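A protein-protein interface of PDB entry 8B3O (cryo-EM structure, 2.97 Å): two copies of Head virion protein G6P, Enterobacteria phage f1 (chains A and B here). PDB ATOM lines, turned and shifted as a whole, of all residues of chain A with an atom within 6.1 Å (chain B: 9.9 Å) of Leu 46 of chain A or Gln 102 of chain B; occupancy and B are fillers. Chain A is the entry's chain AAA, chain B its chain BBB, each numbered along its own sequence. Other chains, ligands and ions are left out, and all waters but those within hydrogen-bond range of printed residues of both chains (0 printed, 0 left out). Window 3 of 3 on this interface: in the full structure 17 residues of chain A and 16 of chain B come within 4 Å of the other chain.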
ATOM      1  N   SER A  41     -34.136 -22.174 -16.681  1.00  0.00           N
ATOM      2  CA  SER A  41     -33.980 -20.754 -16.946  1.00  0.00           C
ATOM      3  C   SER A  41     -32.565 -20.302 -16.592  1.00  0.00           C
ATOM      4  O   SER A  41     -31.880 -19.755 -17.451  1.00  0.00           O
ATOM      5  CB  SER A  41     -35.028 -19.935 -16.238  1.00  0.00           C
ATOM      6  OG  SER A  41     -34.822 -18.549 -16.466  1.00  0.00           O
ATOM      7  N   LEU A  42     -32.126 -20.597 -15.357  1.00  0.00           N
ATOM      8  CA  LEU A  42     -30.832 -20.166 -14.844  1.00  0.00           C
ATOM      9  C   LEU A  42     -29.702 -20.584 -15.782  1.00  0.00           C
ATOM     10  O   LEU A  42     -28.886 -19.748 -16.165  1.00  0.00           O
ATOM     11  CB  LEU A  42     -30.607 -20.725 -13.433  1.00  0.00           C
ATOM     12  CG  LEU A  42     -31.197 -19.913 -12.280  1.00  0.00           C
ATOM     13  CD1 LEU A  42     -30.898 -20.578 -10.945  1.00  0.00           C
ATOM     14  CD2 LEU A  42     -30.661 -18.492 -12.290  1.00  0.00           C
ATOM     15  N   PHE A  43     -29.686 -21.871 -16.152  1.00  0.00           N
ATOM     16  CA  PHE A  43     -28.626 -22.489 -16.937  1.00  0.00           C
ATOM     17  C   PHE A  43     -28.468 -21.764 -18.274  1.00  0.00           C
ATOM     18  O   PHE A  43     -27.379 -21.278 -18.603  1.00  0.00           O
ATOM     19  CB  PHE A  43     -28.868 -24.006 -16.981  1.00  0.00           C
ATOM     20  CG  PHE A  43     -28.433 -24.765 -18.211  1.00  0.00           C
ATOM     21  CD1 PHE A  43     -27.096 -25.077 -18.424  1.00  0.00           C
ATOM     22  CD2 PHE A  43     -29.372 -25.232 -19.124  1.00  0.00           C
ATOM     23  CE1 PHE A  43     -26.706 -25.794 -19.548  1.00  0.00           C
ATOM     24  CE2 PHE A  43     -28.983 -25.949 -20.246  1.00  0.00           C
ATOM     25  CZ  PHE A  43     -27.650 -26.236 -20.453  1.00  0.00           C
ATOM     26  N   LEU A  44     -29.589 -21.641 -18.993  1.00  0.00           N
ATOM     27  CA  LEU A  44     -29.616 -21.012 -20.303  1.00  0.00           C
ATOM     28  C   LEU A  44     -29.292 -19.523 -20.189  1.00  0.00           C
ATOM     29  O   LEU A  44     -28.852 -18.922 -21.164  1.00  0.00           O
ATOM     30  CB  LEU A  44     -30.973 -21.255 -20.975  1.00  0.00           C
ATOM     31  CG  LEU A  44     -31.287 -22.700 -21.369  1.00  0.00           C
ATOM     32  CD1 LEU A  44     -32.735 -22.833 -21.812  1.00  0.00           C
ATOM     33  CD2 LEU A  44     -30.351 -23.203 -22.460  1.00  0.00           C
ATOM     34  N   ALA A  45     -29.466 -18.937 -18.998  1.00  0.00           N
ATOM     35  CA  ALA A  45     -29.173 -17.520 -18.857  1.00  0.00           C
ATOM     36  C   ALA A  45     -27.677 -17.297 -18.638  1.00  0.00           C
ATOM     37  O   ALA A  45     -27.150 -16.244 -18.997  1.00  0.00           O
ATOM     38  CB  ALA A  45     -30.007 -16.900 -17.769  1.00  0.00           C
ATOM     39  N   LEU A  46     -27.007 -18.292 -18.048  1.00  0.00           N
ATOM     40  CA  LEU A  46     -25.578 -18.206 -17.794  1.00  0.00           C
ATOM     41  C   LEU A  46     -24.791 -18.420 -19.087  1.00  0.00           C
ATOM     42  O   LEU A  46     -23.714 -17.849 -19.249  1.00  0.00           O
ATOM     43  CB  LEU A  46     -25.192 -19.186 -16.678  1.00  0.00           C
ATOM     44  CG  LEU A  46     -25.656 -18.777 -15.276  1.00  0.00           C
ATOM     45  CD1 LEU A  46     -25.326 -19.840 -14.243  1.00  0.00           C
ATOM     46  CD2 LEU A  46     -25.061 -17.439 -14.855  1.00  0.00           C
ATOM     47  N   ILE A  47     -25.362 -19.205 -20.011  1.00  0.00           N
ATOM     48  CA  ILE A  47     -24.754 -19.462 -21.309  1.00  0.00           C
ATOM     49  C   ILE A  47     -24.837 -18.199 -22.165  1.00  0.00           C
ATOM     50  O   ILE A  47     -23.819 -17.745 -22.680  1.00  0.00           O
ATOM     51  CB  ILE A  47     -25.364 -20.705 -21.992  1.00  0.00           C
ATOM     52  CG1 ILE A  47     -25.074 -21.978 -21.186  1.00  0.00           C
ATOM     53  CG2 ILE A  47     -24.900 -20.819 -23.441  1.00  0.00           C
ATOM     54  CD1 ILE A  47     -25.277 -23.269 -21.946  1.00  0.00           C
ATOM     55  N   ILE A  48     -26.044 -17.624 -22.279  1.00  0.00           N
ATOM     56  CA  ILE A  48     -26.282 -16.430 -23.081  1.00  0.00           C
ATOM     57  C   ILE A  48     -25.431 -15.276 -22.544  1.00  0.00           C
ATOM     58  O   ILE A  48     -25.034 -14.396 -23.306  1.00  0.00           O
ATOM     59  CB  ILE A  48     -27.792 -16.099 -23.168  1.00  0.00           C
ATOM     60  CG1 ILE A  48     -28.561 -17.180 -23.936  1.00  0.00           C
ATOM     61  CG2 ILE A  48     -28.037 -14.718 -23.767  1.00  0.00           C
ATOM     62  CD1 ILE A  48     -30.071 -17.086 -23.824  1.00  0.00           C
ATOM     63  N   GLY A  49     -25.118 -15.324 -21.240  1.00  0.00           N
ATOM     64  CA  GLY A  49     -24.336 -14.306 -20.556  1.00  0.00           C
ATOM     65  C   GLY A  49     -22.850 -14.348 -20.913  1.00  0.00           C
ATOM     66  O   GLY A  49     -22.245 -13.306 -21.166  1.00  0.00           O
ATOM     67  N   LEU A  50     -22.270 -15.557 -20.908  1.00  0.00           N
ATOM     68  CA  LEU A  50     -20.866 -15.763 -21.231  1.00  0.00           C
ATOM     69  C   LEU A  50     -20.595 -15.325 -22.671  1.00  0.00           C
ATOM     70  O   LEU A  50     -19.579 -14.687 -22.944  1.00  0.00           O
ATOM     71  CB  LEU A  50     -20.504 -17.236 -21.002  1.00  0.00           C
ATOM     72  CG  LEU A  50     -19.029 -17.611 -21.163  1.00  0.00           C
ATOM     73  CD1 LEU A  50     -18.194 -17.097 -19.999  1.00  0.00           C
ATOM     74  CD2 LEU A  50     -18.871 -19.118 -21.297  1.00  0.00           C
ATOM     75  N   ASN A  51     -21.535 -15.638 -23.572  1.00  0.00           N
ATOM     76  CA  ASN A  51     -21.414 -15.291 -24.979  1.00  0.00           C
ATOM     77  C   ASN A  51     -21.113 -13.802 -25.129  1.00  0.00           C
ATOM     78  O   ASN A  51     -20.223 -13.442 -25.893  1.00  0.00           O
ATOM     79  CB  ASN A  51     -22.646 -15.690 -25.796  1.00  0.00           C
ATOM     80  CG  ASN A  51     -22.491 -15.403 -27.275  1.00  0.00           C
ATOM     81  OD1 ASN A  51     -23.112 -14.482 -27.802  1.00  0.00           O
ATOM     82  ND2 ASN A  51     -21.654 -16.175 -27.950  1.00  0.00           N
ATOM     83  N   LYS A 103     -28.940 -31.987 -22.568  1.00  0.00           N
ATOM     84  CA  LYS A 103     -28.990 -31.654 -21.151  1.00  0.00           C
ATOM     85  C   LYS A 103     -30.397 -31.212 -20.738  1.00  0.00           C
ATOM     86  O   LYS A 103     -30.689 -31.136 -19.545  1.00  0.00           O
ATOM     87  CB  LYS A 103     -27.924 -30.611 -20.789  1.00  0.00           C
ATOM     88  CG  LYS A 103     -27.546 -30.553 -19.313  1.00  0.00           C
ATOM     89  CD  LYS A 103     -26.628 -29.406 -18.948  1.00  0.00           C
ATOM     90  CE  LYS A 103     -26.645 -29.086 -17.467  1.00  0.00           C
ATOM     91  NZ  LYS A 103     -25.630 -28.067 -17.106  1.00  0.00           N
ATOM     92  N   PHE B  43     -17.795 -27.049   0.257  1.00  0.00           N
ATOM     93  CA  PHE B  43     -17.250 -27.019  -1.094  1.00  0.00           C
ATOM     94  C   PHE B  43     -16.503 -25.707  -1.331  1.00  0.00           C
ATOM     95  O   PHE B  43     -15.315 -25.710  -1.675  1.00  0.00           O
ATOM     96  CB  PHE B  43     -18.368 -27.379  -2.081  1.00  0.00           C
ATOM     97  CG  PHE B  43     -18.335 -26.764  -3.460  1.00  0.00           C
ATOM     98  CD1 PHE B  43     -17.460 -27.234  -4.432  1.00  0.00           C
ATOM     99  CD2 PHE B  43     -19.230 -25.759  -3.808  1.00  0.00           C
ATOM    100  CE1 PHE B  43     -17.451 -26.676  -5.704  1.00  0.00           C
ATOM    101  CE2 PHE B  43     -19.221 -25.202  -5.080  1.00  0.00           C
ATOM    102  CZ  PHE B  43     -18.335 -25.668  -6.028  1.00  0.00           C
ATOM    103  N   LEU B  44     -17.202 -24.595  -1.070  1.00  0.00           N
ATOM    104  CA  LEU B  44     -16.660 -23.263  -1.275  1.00  0.00           C
ATOM    105  C   LEU B  44     -15.507 -22.998  -0.307  1.00  0.00           C
ATOM    106  O   LEU B  44     -14.668 -22.149  -0.585  1.00  0.00           O
ATOM    107  CB  LEU B  44     -17.774 -22.215  -1.138  1.00  0.00           C
ATOM    108  CG  LEU B  44     -18.856 -22.231  -2.221  1.00  0.00           C
ATOM    109  CD1 LEU B  44     -20.003 -21.308  -1.845  1.00  0.00           C
ATOM    110  CD2 LEU B  44     -18.294 -21.850  -3.585  1.00  0.00           C
ATOM    111  N   ALA B  94     -13.346 -16.060 -16.451  1.00  0.00           N
ATOM    112  CA  ALA B  94     -14.749 -16.161 -16.835  1.00  0.00           C
ATOM    113  C   ALA B  94     -15.261 -17.596 -16.715  1.00  0.00           C
ATOM    114  O   ALA B  94     -16.339 -17.814 -16.168  1.00  0.00           O
ATOM    115  CB  ALA B  94     -14.948 -15.614 -18.228  1.00  0.00           C
ATOM    116  N   ILE B  95     -14.464 -18.565 -17.192  1.00  0.00           N
ATOM    117  CA  ILE B  95     -14.857 -19.968 -17.232  1.00  0.00           C
ATOM    118  C   ILE B  95     -14.925 -20.550 -15.816  1.00  0.00           C
ATOM    119  O   ILE B  95     -15.722 -21.451 -15.571  1.00  0.00           O
ATOM    120  CB  ILE B  95     -13.975 -20.776 -18.216  1.00  0.00           C
ATOM    121  CG1 ILE B  95     -14.281 -20.390 -19.669  1.00  0.00           C
ATOM    122  CG2 ILE B  95     -14.106 -22.280 -18.002  1.00  0.00           C
ATOM    123  CD1 ILE B  95     -13.288 -20.910 -20.693  1.00  0.00           C
ATOM    124  N   PHE B  96     -14.124 -20.008 -14.886  1.00  0.00           N
ATOM    125  CA  PHE B  96     -14.110 -20.442 -13.494  1.00  0.00           C
ATOM    126  C   PHE B  96     -15.362 -19.961 -12.754  1.00  0.00           C
ATOM    127  O   PHE B  96     -15.846 -20.654 -11.858  1.00  0.00           O
ATOM    128  CB  PHE B  96     -12.771 -20.085 -12.833  1.00  0.00           C
ATOM    129  CG  PHE B  96     -12.760 -20.023 -11.325  1.00  0.00           C
ATOM    130  CD1 PHE B  96     -12.611 -21.175 -10.563  1.00  0.00           C
ATOM    131  CD2 PHE B  96     -12.879 -18.804 -10.669  1.00  0.00           C
ATOM    132  CE1 PHE B  96     -12.603 -21.112  -9.175  1.00  0.00           C
ATOM    133  CE2 PHE B  96     -12.867 -18.742  -9.282  1.00  0.00           C
ATOM    134  CZ  PHE B  96     -12.727 -19.895  -8.537  1.00  0.00           C
ATOM    135  N   ILE B  97     -15.888 -18.784 -13.124  1.00  0.00           N
ATOM    136  CA  ILE B  97     -17.106 -18.290 -12.494  1.00  0.00           C
ATOM    137  C   ILE B  97     -18.314 -19.055 -13.039  1.00  0.00           C
ATOM    138  O   ILE B  97     -19.213 -19.398 -12.277  1.00  0.00           O
ATOM    139  CB  ILE B  97     -17.240 -16.753 -12.591  1.00  0.00           C
ATOM    140  CG1 ILE B  97     -16.042 -16.053 -11.943  1.00  0.00           C
ATOM    141  CG2 ILE B  97     -18.551 -16.268 -11.982  1.00  0.00           C
ATOM    142  CD1 ILE B  97     -15.551 -14.842 -12.698  1.00  0.00           C
ATOM    143  N   PHE B  98     -18.308 -19.348 -14.348  1.00  0.00           N
ATOM    144  CA  PHE B  98     -19.346 -20.148 -14.985  1.00  0.00           C
ATOM    145  C   PHE B  98     -19.445 -21.519 -14.312  1.00  0.00           C
ATOM    146  O   PHE B  98     -20.544 -21.972 -14.013  1.00  0.00           O
ATOM    147  CB  PHE B  98     -19.131 -20.204 -16.502  1.00  0.00           C
ATOM    148  CG  PHE B  98     -20.057 -21.107 -17.281  1.00  0.00           C
ATOM    149  CD1 PHE B  98     -21.344 -20.702 -17.620  1.00  0.00           C
ATOM    150  CD2 PHE B  98     -19.630 -22.363 -17.700  1.00  0.00           C
ATOM    151  CE1 PHE B  98     -22.189 -21.540 -18.335  1.00  0.00           C
ATOM    152  CE2 PHE B  98     -20.473 -23.195 -18.426  1.00  0.00           C
ATOM    153  CZ  PHE B  98     -21.750 -22.781 -18.744  1.00  0.00           C
ATOM    154  N   ASP B  99     -18.294 -22.141 -14.025  1.00  0.00           N
ATOM    155  CA  ASP B  99     -18.241 -23.491 -13.480  1.00  0.00           C
ATOM    156  C   ASP B  99     -18.784 -23.553 -12.055  1.00  0.00           C
ATOM    157  O   ASP B  99     -19.535 -24.474 -11.734  1.00  0.00           O
ATOM    158  CB  ASP B  99     -16.832 -24.074 -13.561  1.00  0.00           C
ATOM    159  CG  ASP B  99     -16.418 -24.474 -14.963  1.00  0.00           C
ATOM    160  OD1 ASP B  99     -17.259 -24.376 -15.891  1.00  0.00           O
ATOM    161  OD2 ASP B  99     -15.254 -24.869 -15.110  1.00  0.00           O
ATOM    162  N   VAL B 100     -18.387 -22.592 -11.209  1.00  0.00           N
ATOM    163  CA  VAL B 100     -18.801 -22.548  -9.812  1.00  0.00           C
ATOM    164  C   VAL B 100     -20.311 -22.307  -9.737  1.00  0.00           C
ATOM    165  O   VAL B 100     -21.008 -22.983  -8.981  1.00  0.00           O
ATOM    166  CB  VAL B 100     -17.986 -21.519  -8.994  1.00  0.00           C
ATOM    167  CG1 VAL B 100     -18.561 -21.280  -7.603  1.00  0.00           C
ATOM    168  CG2 VAL B 100     -16.516 -21.902  -8.890  1.00  0.00           C
ATOM    169  N   LYS B 101     -20.806 -21.366 -10.554  1.00  0.00           N
ATOM    170  CA  LYS B 101     -22.211 -20.983 -10.559  1.00  0.00           C
ATOM    171  C   LYS B 101     -23.097 -22.088 -11.140  1.00  0.00           C
ATOM    172  O   LYS B 101     -24.267 -22.166 -10.776  1.00  0.00           O
ATOM    173  CB  LYS B 101     -22.418 -19.628 -11.243  1.00  0.00           C
ATOM    174  CG  LYS B 101     -22.245 -18.416 -10.338  1.00  0.00           C
ATOM    175  CD  LYS B 101     -22.111 -17.116 -11.099  1.00  0.00           C
ATOM    176  CE  LYS B 101     -21.942 -15.920 -10.187  1.00  0.00           C
ATOM    177  NZ  LYS B 101     -22.251 -14.650 -10.884  1.00  0.00           N
ATOM    178  N   GLN B 102     -22.546 -22.935 -12.028  1.00  0.00           N
ATOM    179  CA  GLN B 102     -23.286 -24.043 -12.621  1.00  0.00           C
ATOM    180  C   GLN B 102     -23.450 -25.204 -11.635  1.00  0.00           C
ATOM    181  O   GLN B 102     -24.334 -26.038 -11.827  1.00  0.00           O
ATOM    182  CB  GLN B 102     -22.640 -24.516 -13.927  1.00  0.00           C
ATOM    183  CG  GLN B 102     -22.947 -23.621 -15.119  1.00  0.00           C
ATOM    184  CD  GLN B 102     -24.384 -23.746 -15.553  1.00  0.00           C
ATOM    185  OE1 GLN B 102     -24.809 -24.774 -16.076  1.00  0.00           O
ATOM    186  NE2 GLN B 102     -25.155 -22.695 -15.338  1.00  0.00           N
ATOM    187  N   LYS B 103     -22.598 -25.255 -10.598  1.00  0.00           N
ATOM    188  CA  LYS B 103     -22.620 -26.329  -9.612  1.00  0.00           C
ATOM    189  C   LYS B 103     -23.494 -25.959  -8.411  1.00  0.00           C
ATOM    190  O   LYS B 103     -23.831 -26.827  -7.608  1.00  0.00           O
ATOM    191  CB  LYS B 103     -21.198 -26.728  -9.195  1.00  0.00           C
ATOM    192  CG  LYS B 103     -21.066 -28.118  -8.579  1.00  0.00           C
ATOM    193  CD  LYS B 103     -19.695 -28.421  -8.015  1.00  0.00           C
ATOM    194  CE  LYS B 103     -19.706 -29.566  -7.024  1.00  0.00           C
ATOM    195  NZ  LYS B 103     -18.338 -29.947  -6.598  1.00  0.00           N
ATOM    196  N   ILE B 104     -23.862 -24.676  -8.291  1.00  0.00           N
ATOM    197  CA  ILE B 104     -24.751 -24.232  -7.224  1.00  0.00           C
ATOM    198  C   ILE B 104     -26.211 -24.434  -7.645  1.00  0.00           C
ATOM    199  O   ILE B 104     -27.081 -24.566  -6.786  1.00  0.00           O
ATOM    200  CB  ILE B 104     -24.413 -22.795  -6.758  1.00  0.00           C
ATOM    201  CG1 ILE B 104     -23.011 -22.742  -6.138  1.00  0.00           C
ATOM    202  CG2 ILE B 104     -25.468 -22.238  -5.806  1.00  0.00           C
ATOM    203  CD1 ILE B 104     -22.611 -21.397  -5.575  1.00  0.00           C
ATOM    204  N   VAL B 105     -26.461 -24.510  -8.960  1.00  0.00           N
ATOM    205  CA  VAL B 105     -27.794 -24.711  -9.515  1.00  0.00           C
ATOM    206  C   VAL B 105     -28.132 -26.206  -9.524  1.00  0.00           C
ATOM    207  O   VAL B 105     -29.291 -26.584  -9.702  1.00  0.00           O
ATOM    208  CB  VAL B 105     -27.930 -24.055 -10.908  1.00  0.00           C
ATOM    209  CG1 VAL B 105     -29.324 -24.197 -11.503  1.00  0.00           C
ATOM    210  CG2 VAL B 105     -27.532 -22.588 -10.880  1.00  0.00           C
ATOM    211  N   SER B 106     -27.117 -27.055  -9.313  1.00  0.00           N
ATOM    212  CA  SER B 106     -27.302 -28.499  -9.278  1.00  0.00           C
ATOM    213  C   SER B 106     -27.635 -28.982  -7.866  1.00  0.00           C
ATOM    214  O   SER B 106     -27.996 -30.144  -7.687  1.00  0.00           O
ATOM    215  CB  SER B 106     -26.102 -29.214  -9.848  1.00  0.00           C
ATOM    216  OG  SER B 106     -26.252 -30.622  -9.736  1.00  0.00           O
ATOM    217  N   TYR B 107     -27.521 -28.083  -6.877  1.00  0.00           N
ATOM    218  CA  TYR B 107     -27.878 -28.392  -5.500  1.00  0.00           C
ATOM    219  C   TYR B 107     -29.394 -28.315  -5.310  1.00  0.00           C
ATOM    220  O   TYR B 107     -29.901 -28.659  -4.242  1.00  0.00           O
ATOM    221  CB  TYR B 107     -27.110 -27.509  -4.511  1.00  0.00           C
ATOM    222  CG  TYR B 107     -25.725 -27.998  -4.164  1.00  0.00           C
ATOM    223  CD1 TYR B 107     -25.537 -29.114  -3.358  1.00  0.00           C
ATOM    224  CD2 TYR B 107     -24.597 -27.333  -4.625  1.00  0.00           C
ATOM    225  CE1 TYR B 107     -24.266 -29.567  -3.036  1.00  0.00           C
ATOM    226  CE2 TYR B 107     -23.319 -27.774  -4.313  1.00  0.00           C
ATOM    227  CZ  TYR B 107     -23.154 -28.894  -3.514  1.00  0.00           C
ATOM    228  OH  TYR B 107     -21.901 -29.334  -3.199  1.00  0.00           O
ATOM    229  N   LEU B 108     -30.106 -27.883  -6.359  1.00  0.00           N
ATOM    230  CA  LEU B 108     -31.558 -27.795  -6.339  1.00  0.00           C
ATOM    231  C   LEU B 108     -32.192 -29.172  -6.536  1.00  0.00           C
ATOM    232  O   LEU B 108     -33.414 -29.292  -6.494  1.00  0.00           O
ATOM    233  CB  LEU B 108     -32.030 -26.801  -7.409  1.00  0.00           C
ATOM    234  CG  LEU B 108     -32.123 -25.339  -6.973  1.00  0.00           C
ATOM    235  CD1 LEU B 108     -32.516 -24.450  -8.143  1.00  0.00           C
ATOM    236  CD2 LEU B 108     -33.109 -25.160  -5.827  1.00  0.00           C
ATOM    237  N   ASP B 109     -31.355 -30.202  -6.734  1.00  0.00           N
ATOM    238  CA  ASP B 109     -31.816 -31.567  -6.939  1.00  0.00           C
ATOM    239  C   ASP B 109     -31.491 -32.428  -5.717  1.00  0.00           C
ATOM    240  O   ASP B 109     -31.705 -33.640  -5.731  1.00  0.00           O
ATOM    241  CB  ASP B 109     -31.262 -32.148  -8.244  1.00  0.00           C
ATOM    242  CG  ASP B 109     -32.101 -33.280  -8.814  1.00  0.00           C
ATOM    243  OD1 ASP B 109     -33.344 -33.147  -8.822  1.00  0.00           O
ATOM    244  OD2 ASP B 109     -31.506 -34.289  -9.245  1.00  0.00           O
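Of chain B, only Gln 102 comes within 4 Å of Leu 46 of chain A.
No residue of chain B comes within 4 Å of Ala 45 of chain A.
No residue of chain B comes within 4 Å of Ile 47 of chain A.
No residue of chain B comes within 4 Å of Gly 49 of chain A.
Of the printed residues of chain B, Leu 50 of chain A touches Ala 94.
Printed residues of chain B within 4 Å of Leu 42 of chain A: Val 105.
Printed residues of chain A within 4 Å of Val 105 of chain B: Leu 42.
Ile 97 of chain B touches none of the printed residues of chain A.
Ser 106 of chain B touches none of the printed residues of chain A.
The nearest printed residue of chain B that does not touch Phe 43 of chain A is Phe 98 of chain B (5.2 Å).
CD1 of Leu 42 of chain A touches CG2 of Val 105 of chain B, at 3.9 Å.
Gln 102 of chain B touches Phe 43 of chain A.
Leu 46 of chain A touches Gln 102 of chain B.
Leu 50 of chain A touches Ala 94 of chain B.
NZ of Lys 103 of chain A touches OE1 of Gln 102 of chain B, at 3.5 Å.
Hydrophobic or aromatic side chains of chain A within 4 Å of the printed part of chain B: Leu 42, Phe 43, Leu 46 and Leu 50.
Hydrophobic or aromatic side chains of chain B that line the printed part of chain A: Ala 94 and Val 105.
Among the printed residues, 5 pairs touch across the chains.
3 positions are printed for both chains.
Of the 5 pairs that touch across the chains among the printed residues, none has its exchanged pair printed and touching as well.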
